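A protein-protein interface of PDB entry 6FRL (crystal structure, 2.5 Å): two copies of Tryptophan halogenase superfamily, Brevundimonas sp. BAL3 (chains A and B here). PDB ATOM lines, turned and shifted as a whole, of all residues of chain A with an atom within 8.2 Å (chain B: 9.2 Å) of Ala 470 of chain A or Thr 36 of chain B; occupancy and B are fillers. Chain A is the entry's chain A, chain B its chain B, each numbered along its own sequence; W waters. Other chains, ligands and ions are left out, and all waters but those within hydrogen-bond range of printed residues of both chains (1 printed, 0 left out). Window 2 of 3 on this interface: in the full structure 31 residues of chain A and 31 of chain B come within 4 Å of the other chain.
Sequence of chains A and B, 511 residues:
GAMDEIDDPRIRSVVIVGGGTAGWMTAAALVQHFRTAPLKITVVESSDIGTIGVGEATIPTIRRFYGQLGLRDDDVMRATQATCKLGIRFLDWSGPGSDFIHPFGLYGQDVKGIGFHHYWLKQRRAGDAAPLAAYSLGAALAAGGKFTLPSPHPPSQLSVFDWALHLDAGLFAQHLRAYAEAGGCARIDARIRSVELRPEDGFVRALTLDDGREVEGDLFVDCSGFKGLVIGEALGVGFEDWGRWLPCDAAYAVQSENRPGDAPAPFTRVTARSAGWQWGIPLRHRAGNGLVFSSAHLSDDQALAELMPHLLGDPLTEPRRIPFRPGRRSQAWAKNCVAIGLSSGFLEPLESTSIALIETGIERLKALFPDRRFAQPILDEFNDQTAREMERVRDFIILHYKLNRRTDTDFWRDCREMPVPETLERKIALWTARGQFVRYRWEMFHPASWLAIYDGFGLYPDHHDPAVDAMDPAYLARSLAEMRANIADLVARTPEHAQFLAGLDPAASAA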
ATOM      1  N   LYS A 112      29.964 -11.491 -30.872  1.00  0.00           N
ATOM      2  CA  LYS A 112      28.562 -11.906 -30.982  1.00  0.00           C
ATOM      3  C   LYS A 112      27.569 -10.837 -30.497  1.00  0.00           C
ATOM      4  O   LYS A 112      26.508 -11.161 -29.946  1.00  0.00           O
ATOM      5  CB  LYS A 112      28.349 -13.247 -30.249  1.00  0.00           C
ATOM      6  CG  LYS A 112      29.119 -14.394 -30.899  1.00  0.00           C
ATOM      7  CD  LYS A 112      28.838 -15.752 -30.279  1.00  0.00           C
ATOM      8  CE  LYS A 112      29.327 -16.870 -31.195  1.00  0.00           C
ATOM      9  NZ  LYS A 112      28.971 -18.210 -30.662  1.00  0.00           N
ATOM     10  N   TYR A 119      33.127 -10.645 -21.145  1.00  0.00           N
ATOM     11  CA  TYR A 119      34.089 -11.749 -21.239  1.00  0.00           C
ATOM     12  C   TYR A 119      35.256 -11.510 -20.274  1.00  0.00           C
ATOM     13  O   TYR A 119      35.649 -12.427 -19.547  1.00  0.00           O
ATOM     14  CB  TYR A 119      34.580 -11.939 -22.663  1.00  0.00           C
ATOM     15  CG  TYR A 119      33.484 -12.292 -23.650  1.00  0.00           C
ATOM     16  CD1 TYR A 119      33.094 -13.611 -23.852  1.00  0.00           C
ATOM     17  CD2 TYR A 119      32.833 -11.283 -24.394  1.00  0.00           C
ATOM     18  CE1 TYR A 119      32.080 -13.931 -24.768  1.00  0.00           C
ATOM     19  CE2 TYR A 119      31.819 -11.579 -25.293  1.00  0.00           C
ATOM     20  CZ  TYR A 119      31.457 -12.906 -25.501  1.00  0.00           C
ATOM     21  OH  TYR A 119      30.471 -13.179 -26.419  1.00  0.00           O
ATOM     22  N   LYS A 122      34.004 -12.392 -16.720  1.00  0.00           N
ATOM     23  CA  LYS A 122      33.958 -13.853 -16.554  1.00  0.00           C
ATOM     24  C   LYS A 122      35.326 -14.390 -16.192  1.00  0.00           C
ATOM     25  O   LYS A 122      35.470 -15.123 -15.202  1.00  0.00           O
ATOM     26  CB  LYS A 122      33.459 -14.574 -17.825  1.00  0.00           C
ATOM     27  CG  LYS A 122      33.723 -16.069 -17.812  1.00  0.00           C
ATOM     28  CD  LYS A 122      33.376 -16.816 -19.077  1.00  0.00           C
ATOM     29  CE  LYS A 122      33.227 -18.324 -18.777  1.00  0.00           C
ATOM     30  NZ  LYS A 122      34.026 -18.919 -17.640  1.00  0.00           N
ATOM     31  N   HIS A 464      27.712 -10.605 -14.818  1.00  0.00           N
ATOM     32  CA  HIS A 464      27.932 -10.329 -16.282  1.00  0.00           C
ATOM     33  C   HIS A 464      26.805 -10.989 -17.147  1.00  0.00           C
ATOM     34  O   HIS A 464      25.923 -11.667 -16.607  1.00  0.00           O
ATOM     35  CB  HIS A 464      29.351 -10.758 -16.768  1.00  0.00           C
ATOM     36  CG  HIS A 464      29.652 -12.214 -16.568  1.00  0.00           C
ATOM     37  ND1 HIS A 464      30.452 -12.669 -15.542  1.00  0.00           N
ATOM     38  CD2 HIS A 464      29.235 -13.320 -17.235  1.00  0.00           C
ATOM     39  CE1 HIS A 464      30.527 -13.991 -15.596  1.00  0.00           C
ATOM     40  NE2 HIS A 464      29.795 -14.410 -16.615  1.00  0.00           N
ATOM     41  N   ASP A 465      26.844 -10.782 -18.467  1.00  0.00           N
ATOM     42  CA  ASP A 465      25.847 -11.333 -19.417  1.00  0.00           C
ATOM     43  C   ASP A 465      25.974 -12.880 -19.511  1.00  0.00           C
ATOM     44  O   ASP A 465      27.045 -13.347 -19.860  1.00  0.00           O
ATOM     45  CB  ASP A 465      26.092 -10.649 -20.779  1.00  0.00           C
ATOM     46  CG  ASP A 465      25.052 -10.987 -21.838  1.00  0.00           C
ATOM     47  OD1 ASP A 465      24.527 -12.130 -21.898  1.00  0.00           O
ATOM     48  OD2 ASP A 465      24.799 -10.084 -22.658  1.00  0.00           O
ATOM     49  N   PRO A 466      24.900 -13.667 -19.224  1.00  0.00           N
ATOM     50  CA  PRO A 466      25.081 -15.144 -19.086  1.00  0.00           C
ATOM     51  C   PRO A 466      25.276 -15.940 -20.374  1.00  0.00           C
ATOM     52  O   PRO A 466      25.487 -17.148 -20.295  1.00  0.00           O
ATOM     53  CB  PRO A 466      23.786 -15.611 -18.414  1.00  0.00           C
ATOM     54  CG  PRO A 466      22.784 -14.604 -18.832  1.00  0.00           C
ATOM     55  CD  PRO A 466      23.486 -13.279 -19.070  1.00  0.00           C
ATOM     56  N   ALA A 467      25.187 -15.301 -21.544  1.00  0.00           N
ATOM     57  CA  ALA A 467      25.551 -15.967 -22.823  1.00  0.00           C
ATOM     58  C   ALA A 467      27.057 -16.211 -22.911  1.00  0.00           C
ATOM     59  O   ALA A 467      27.519 -17.080 -23.661  1.00  0.00           O
ATOM     60  CB  ALA A 467      25.078 -15.142 -24.023  1.00  0.00           C
ATOM     61  N   VAL A 468      27.788 -15.429 -22.119  1.00  0.00           N
ATOM     62  CA  VAL A 468      29.237 -15.446 -22.029  1.00  0.00           C
ATOM     63  C   VAL A 468      29.771 -16.689 -21.332  1.00  0.00           C
ATOM     64  O   VAL A 468      30.835 -17.160 -21.728  1.00  0.00           O
ATOM     65  CB  VAL A 468      29.728 -14.163 -21.305  1.00  0.00           C
ATOM     66  CG1 VAL A 468      31.191 -14.221 -20.945  1.00  0.00           C
ATOM     67  CG2 VAL A 468      29.453 -12.945 -22.177  1.00  0.00           C
ATOM     68  N   ASP A 469      29.049 -17.198 -20.320  1.00  0.00           N
ATOM     69  CA  ASP A 469      29.427 -18.444 -19.605  1.00  0.00           C
ATOM     70  C   ASP A 469      29.365 -19.740 -20.434  1.00  0.00           C
ATOM     71  O   ASP A 469      29.920 -20.758 -20.017  1.00  0.00           O
ATOM     72  CB  ASP A 469      28.608 -18.621 -18.331  1.00  0.00           C
ATOM     73  CG  ASP A 469      28.858 -17.517 -17.311  1.00  0.00           C
ATOM     74  OD1 ASP A 469      30.030 -17.194 -17.033  1.00  0.00           O
ATOM     75  OD2 ASP A 469      27.883 -16.971 -16.781  1.00  0.00           O
ATOM     76  N   ALA A 470      28.710 -19.673 -21.601  1.00  0.00           N
ATOM     77  CA  ALA A 470      28.756 -20.724 -22.636  1.00  0.00           C
ATOM     78  C   ALA A 470      30.170 -21.001 -23.215  1.00  0.00           C
ATOM     79  O   ALA A 470      30.410 -22.089 -23.760  1.00  0.00           O
ATOM     80  CB  ALA A 470      27.787 -20.364 -23.778  1.00  0.00           C
ATOM     81  N   MET A 471      31.081 -20.025 -23.119  1.00  0.00           N
ATOM     82  CA  MET A 471      32.427 -20.122 -23.705  1.00  0.00           C
ATOM     83  C   MET A 471      33.411 -20.901 -22.802  1.00  0.00           C
ATOM     84  O   MET A 471      33.335 -20.810 -21.564  1.00  0.00           O
ATOM     85  CB  MET A 471      32.952 -18.704 -24.013  1.00  0.00           C
ATOM     86  CG  MET A 471      34.099 -18.637 -25.021  1.00  0.00           C
ATOM     87  SD  MET A 471      34.211 -17.064 -25.869  1.00  0.00           S
ATOM     88  CE  MET A 471      35.978 -16.804 -25.928  1.00  0.00           C
ATOM     89  N   ASP A 472      34.319 -21.647 -23.440  1.00  0.00           N
ATOM     90  CA  ASP A 472      35.265 -22.515 -22.756  1.00  0.00           C
ATOM     91  C   ASP A 472      36.405 -21.690 -22.108  1.00  0.00           C
ATOM     92  O   ASP A 472      37.062 -20.911 -22.810  1.00  0.00           O
ATOM     93  CB  ASP A 472      35.852 -23.527 -23.766  1.00  0.00           C
ATOM     94  CG  ASP A 472      36.728 -24.600 -23.099  1.00  0.00           C
ATOM     95  OD1 ASP A 472      36.194 -25.414 -22.327  1.00  0.00           O
ATOM     96  OD2 ASP A 472      37.952 -24.629 -23.339  1.00  0.00           O
ATOM     97  N   PRO A 473      36.667 -21.882 -20.783  1.00  0.00           N
ATOM     98  CA  PRO A 473      37.676 -21.032 -20.090  1.00  0.00           C
ATOM     99  C   PRO A 473      39.118 -21.178 -20.619  1.00  0.00           C
ATOM    100  O   PRO A 473      39.880 -20.224 -20.540  1.00  0.00           O
ATOM    101  CB  PRO A 473      37.579 -21.471 -18.618  1.00  0.00           C
ATOM    102  CG  PRO A 473      37.007 -22.845 -18.666  1.00  0.00           C
ATOM    103  CD  PRO A 473      36.122 -22.928 -19.889  1.00  0.00           C
ATOM    104  N   ARG B  10      22.094 -17.745 -11.851  1.00  0.00           N
ATOM    105  CA  ARG B  10      21.796 -18.255 -13.202  1.00  0.00           C
ATOM    106  C   ARG B  10      20.343 -18.705 -13.495  1.00  0.00           C
ATOM    107  O   ARG B  10      19.800 -19.578 -12.804  1.00  0.00           O
ATOM    108  CB  ARG B  10      22.743 -19.458 -13.465  1.00  0.00           C
ATOM    109  CG  ARG B  10      23.052 -19.758 -14.919  1.00  0.00           C
ATOM    110  CD  ARG B  10      23.863 -21.062 -15.092  1.00  0.00           C
ATOM    111  NE  ARG B  10      25.261 -20.988 -14.644  1.00  0.00           N
ATOM    112  CZ  ARG B  10      26.220 -20.252 -15.217  1.00  0.00           C
ATOM    113  NH1 ARG B  10      25.969 -19.488 -16.284  1.00  0.00           N
ATOM    114  NH2 ARG B  10      27.458 -20.269 -14.719  1.00  0.00           N
ATOM    115  N   LEU B  30      16.754 -17.056 -28.852  1.00  0.00           N
ATOM    116  CA  LEU B  30      17.348 -17.533 -27.601  1.00  0.00           C
ATOM    117  C   LEU B  30      18.115 -18.870 -27.769  1.00  0.00           C
ATOM    118  O   LEU B  30      19.162 -19.073 -27.128  1.00  0.00           O
ATOM    119  CB  LEU B  30      16.281 -17.635 -26.498  1.00  0.00           C
ATOM    120  CG  LEU B  30      15.606 -16.324 -26.097  1.00  0.00           C
ATOM    121  CD1 LEU B  30      14.614 -16.534 -24.961  1.00  0.00           C
ATOM    122  CD2 LEU B  30      16.652 -15.266 -25.717  1.00  0.00           C
ATOM    123  N   VAL B  31      17.620 -19.763 -28.628  1.00  0.00           N
ATOM    124  CA  VAL B  31      18.363 -20.991 -28.961  1.00  0.00           C
ATOM    125  C   VAL B  31      19.757 -20.657 -29.503  1.00  0.00           C
ATOM    126  O   VAL B  31      20.744 -21.162 -28.986  1.00  0.00           O
ATOM    127  CB  VAL B  31      17.537 -21.930 -29.900  1.00  0.00           C
ATOM    128  CG1 VAL B  31      18.403 -22.901 -30.689  1.00  0.00           C
ATOM    129  CG2 VAL B  31      16.514 -22.726 -29.080  1.00  0.00           C
ATOM    130  N   GLN B  32      19.849 -19.767 -30.493  1.00  0.00           N
ATOM    131  CA  GLN B  32      21.168 -19.392 -31.060  1.00  0.00           C
ATOM    132  C   GLN B  32      22.084 -18.698 -30.034  1.00  0.00           C
ATOM    133  O   GLN B  32      23.267 -18.951 -29.980  1.00  0.00           O
ATOM    134  CB  GLN B  32      21.014 -18.443 -32.262  1.00  0.00           C
ATOM    135  CG  GLN B  32      22.337 -17.912 -32.844  1.00  0.00           C
ATOM    136  CD  GLN B  32      22.953 -18.848 -33.835  1.00  0.00           C
ATOM    137  OE1 GLN B  32      23.033 -20.065 -33.605  1.00  0.00           O
ATOM    138  NE2 GLN B  32      23.389 -18.301 -34.972  1.00  0.00           N
ATOM    139  N   HIS B  33      21.511 -17.781 -29.272  1.00  0.00           N
ATOM    140  CA  HIS B  33      22.281 -16.949 -28.368  1.00  0.00           C
ATOM    141  C   HIS B  33      22.837 -17.741 -27.170  1.00  0.00           C
ATOM    142  O   HIS B  33      23.897 -17.450 -26.697  1.00  0.00           O
ATOM    143  CB  HIS B  33      21.386 -15.821 -27.897  1.00  0.00           C
ATOM    144  CG  HIS B  33      22.093 -14.752 -27.150  1.00  0.00           C
ATOM    145  ND1 HIS B  33      21.734 -14.363 -25.867  1.00  0.00           N
ATOM    146  CD2 HIS B  33      23.099 -13.939 -27.527  1.00  0.00           C
ATOM    147  CE1 HIS B  33      22.503 -13.358 -25.492  1.00  0.00           C
ATOM    148  NE2 HIS B  33      23.344 -13.088 -26.478  1.00  0.00           N
ATOM    149  N   PHE B  34      22.085 -18.732 -26.699  1.00  0.00           N
ATOM    150  CA  PHE B  34      22.467 -19.595 -25.591  1.00  0.00           C
ATOM    151  C   PHE B  34      22.676 -21.054 -26.078  1.00  0.00           C
ATOM    152  O   PHE B  34      22.371 -22.001 -25.323  1.00  0.00           O
ATOM    153  CB  PHE B  34      21.336 -19.599 -24.532  1.00  0.00           C
ATOM    154  CG  PHE B  34      21.151 -18.305 -23.792  1.00  0.00           C
ATOM    155  CD1 PHE B  34      22.068 -17.909 -22.830  1.00  0.00           C
ATOM    156  CD2 PHE B  34      20.022 -17.515 -23.990  1.00  0.00           C
ATOM    157  CE1 PHE B  34      21.880 -16.730 -22.100  1.00  0.00           C
ATOM    158  CE2 PHE B  34      19.845 -16.319 -23.279  1.00  0.00           C
ATOM    159  CZ  PHE B  34      20.781 -15.916 -22.348  1.00  0.00           C
ATOM    160  N   ARG B  35      23.209 -21.246 -27.298  1.00  0.00           N
ATOM    161  CA  ARG B  35      23.247 -22.578 -27.961  1.00  0.00           C
ATOM    162  C   ARG B  35      23.896 -23.702 -27.134  1.00  0.00           C
ATOM    163  O   ARG B  35      23.285 -24.756 -26.944  1.00  0.00           O
ATOM    164  CB  ARG B  35      23.905 -22.508 -29.359  1.00  0.00           C
ATOM    165  CG  ARG B  35      23.613 -23.742 -30.244  1.00  0.00           C
ATOM    166  CD  ARG B  35      24.039 -23.491 -31.695  1.00  0.00           C
ATOM    167  NE  ARG B  35      23.068 -22.785 -32.533  1.00  0.00           N
ATOM    168  CZ  ARG B  35      21.958 -23.323 -33.033  1.00  0.00           C
ATOM    169  NH1 ARG B  35      21.622 -24.578 -32.783  1.00  0.00           N
ATOM    170  NH2 ARG B  35      21.145 -22.609 -33.791  1.00  0.00           N
ATOM    171  N   THR B  36      25.098 -23.450 -26.616  1.00  0.00           N
ATOM    172  CA  THR B  36      25.859 -24.443 -25.829  1.00  0.00           C
ATOM    173  C   THR B  36      25.853 -24.188 -24.310  1.00  0.00           C
ATOM    174  O   THR B  36      26.742 -24.669 -23.602  1.00  0.00           O
ATOM    175  CB  THR B  36      27.338 -24.470 -26.290  1.00  0.00           C
ATOM    176  OG1 THR B  36      27.974 -23.236 -25.917  1.00  0.00           O
ATOM    177  CG2 THR B  36      27.435 -24.646 -27.820  1.00  0.00           C
ATOM    178  N   ALA B  37      24.872 -23.445 -23.804  1.00  0.00           N
ATOM    179  CA  ALA B  37      24.747 -23.168 -22.372  1.00  0.00           C
ATOM    180  C   ALA B  37      23.707 -24.095 -21.794  1.00  0.00           C
ATOM    181  O   ALA B  37      22.853 -24.587 -22.532  1.00  0.00           O
ATOM    182  CB  ALA B  37      24.341 -21.722 -22.140  1.00  0.00           C
ATOM    183  N   PRO B  38      23.751 -24.337 -20.469  1.00  0.00           N
ATOM    184  CA  PRO B  38      22.760 -25.225 -19.887  1.00  0.00           C
ATOM    185  C   PRO B  38      21.521 -24.412 -19.611  1.00  0.00           C
ATOM    186  O   PRO B  38      21.344 -23.934 -18.502  1.00  0.00           O
ATOM    187  CB  PRO B  38      23.439 -25.692 -18.594  1.00  0.00           C
ATOM    188  CG  PRO B  38      24.305 -24.557 -18.191  1.00  0.00           C
ATOM    189  CD  PRO B  38      24.642 -23.778 -19.428  1.00  0.00           C
ATOM    190  N   LEU B  39      20.720 -24.191 -20.644  1.00  0.00           N
ATOM    191  CA  LEU B  39      19.511 -23.394 -20.538  1.00  0.00           C
ATOM    192  C   LEU B  39      18.430 -24.184 -21.234  1.00  0.00           C
ATOM    193  O   LEU B  39      18.547 -24.448 -22.440  1.00  0.00           O
ATOM    194  CB  LEU B  39      19.668 -22.018 -21.194  1.00  0.00           C
ATOM    195  CG  LEU B  39      18.454 -21.071 -21.076  1.00  0.00           C
ATOM    196  CD1 LEU B  39      18.272 -20.638 -19.644  1.00  0.00           C
ATOM    197  CD2 LEU B  39      18.565 -19.831 -21.932  1.00  0.00           C
ATOM    198  N   ILE B  41      14.886 -24.385 -22.904  1.00  0.00           N
ATOM    199  CA  ILE B  41      13.900 -23.539 -23.512  1.00  0.00           C
ATOM    200  C   ILE B  41      12.771 -24.437 -23.982  1.00  0.00           C
ATOM    201  O   ILE B  41      12.999 -25.472 -24.631  1.00  0.00           O
ATOM    202  CB  ILE B  41      14.489 -22.733 -24.694  1.00  0.00           C
ATOM    203  CG1 ILE B  41      15.677 -21.858 -24.230  1.00  0.00           C
ATOM    204  CG2 ILE B  41      13.406 -21.870 -25.347  1.00  0.00           C
ATOM    205  CD1 ILE B  41      16.509 -21.313 -25.368  1.00  0.00           C
ATOM    206  N   GLY B 183      17.986 -27.034 -32.338  1.00  0.00           N
ATOM    207  CA  GLY B 183      18.937 -26.587 -31.306  1.00  0.00           C
ATOM    208  C   GLY B 183      18.561 -26.973 -29.868  1.00  0.00           C
ATOM    209  O   GLY B 183      19.250 -26.571 -28.915  1.00  0.00           O
HETATM  210  O   HOH W   1      23.709 -10.067 -24.855  1.00  0.00           O
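The side-chain carboxylate (OD2) of Asp 469 of chain A lies within salt-bridge range of the guanidinium group (NH1) of Arg 10 of chain B (3.2 Å). The backbone carbonyl oxygen (O) of Ala 470 of chain A sits at hydrogen-bond distance from the side-chain hydroxyl (OG1) of Thr 36 of chain B, 3.4 Å away.
A ring nitrogen (NE2) of His 464 of chain A sits at hydrogen-bond distance from the side-chain carboxylate (OD1) of Asp 469 of chain A (2.8 Å). The side-chain carboxylate (OD1) of Asp 465 of chain A sits close to the backbone NH (N) of Ala 467 of chain A, at 3.3 Å.
C of Pro 466 of chain A touches CE1 of Phe 34 of chain B (3.9 Å). Ala 467 of chain A touches His 33 of chain B (CB to CE1, 3.5 Å). Ala 467 of chain A touches Phe 34 of chain B (N to CE1, 3.6 Å).
Of chain B, only Thr 36 comes within 4 Å of Ala 470 of chain A. Of the printed residues of chain A, Arg 10 of chain B touches Asp 469 (3.2 Å). Printed residues of chain A within 4 Å of His 33 of chain B: Ala 467 (3.5 Å). Of the printed residues of chain A, Phe 34 of chain B touches Pro 466 (3.9 Å) and Ala 467 (3.6 Å). Thr 36 of chain B touches one residue of chain A. No residue of chain A comes within 4 Å of Ala 37 of chain B. The nearest residue of chain B that does not touch Ala 470 of chain A is Ala 37 of chain B (4.05 Å). The nearest residue of chain A that does not touch Thr 36 of chain B is Met 471 of chain A (5.3 Å). The nearest printed residue of chain A that does not touch Phe 34 of chain B is Asp 465 of chain A (5.3 Å).
Of the 13 printed residues of chain A, 4 touch a printed residue of chain B. Along chain B the printed residues that touch a printed residue of chain A span positions 10 to 36. Among the printed residues, 5 pairs touch across the chains. Among the printed residues, Asp or Glu carboxylates within 4 Å of a Lys or Arg side-chain nitrogen of the other chain: Asp 469 of chain A with Arg 10 of chain B (3.2 Å).
No position is printed for both chains.
Water W1 lies within hydrogen-bond range of OD2 of Asp 465 of chain A (2.5 Å) and NE2 of His 33 of chain B (3.4 Å).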
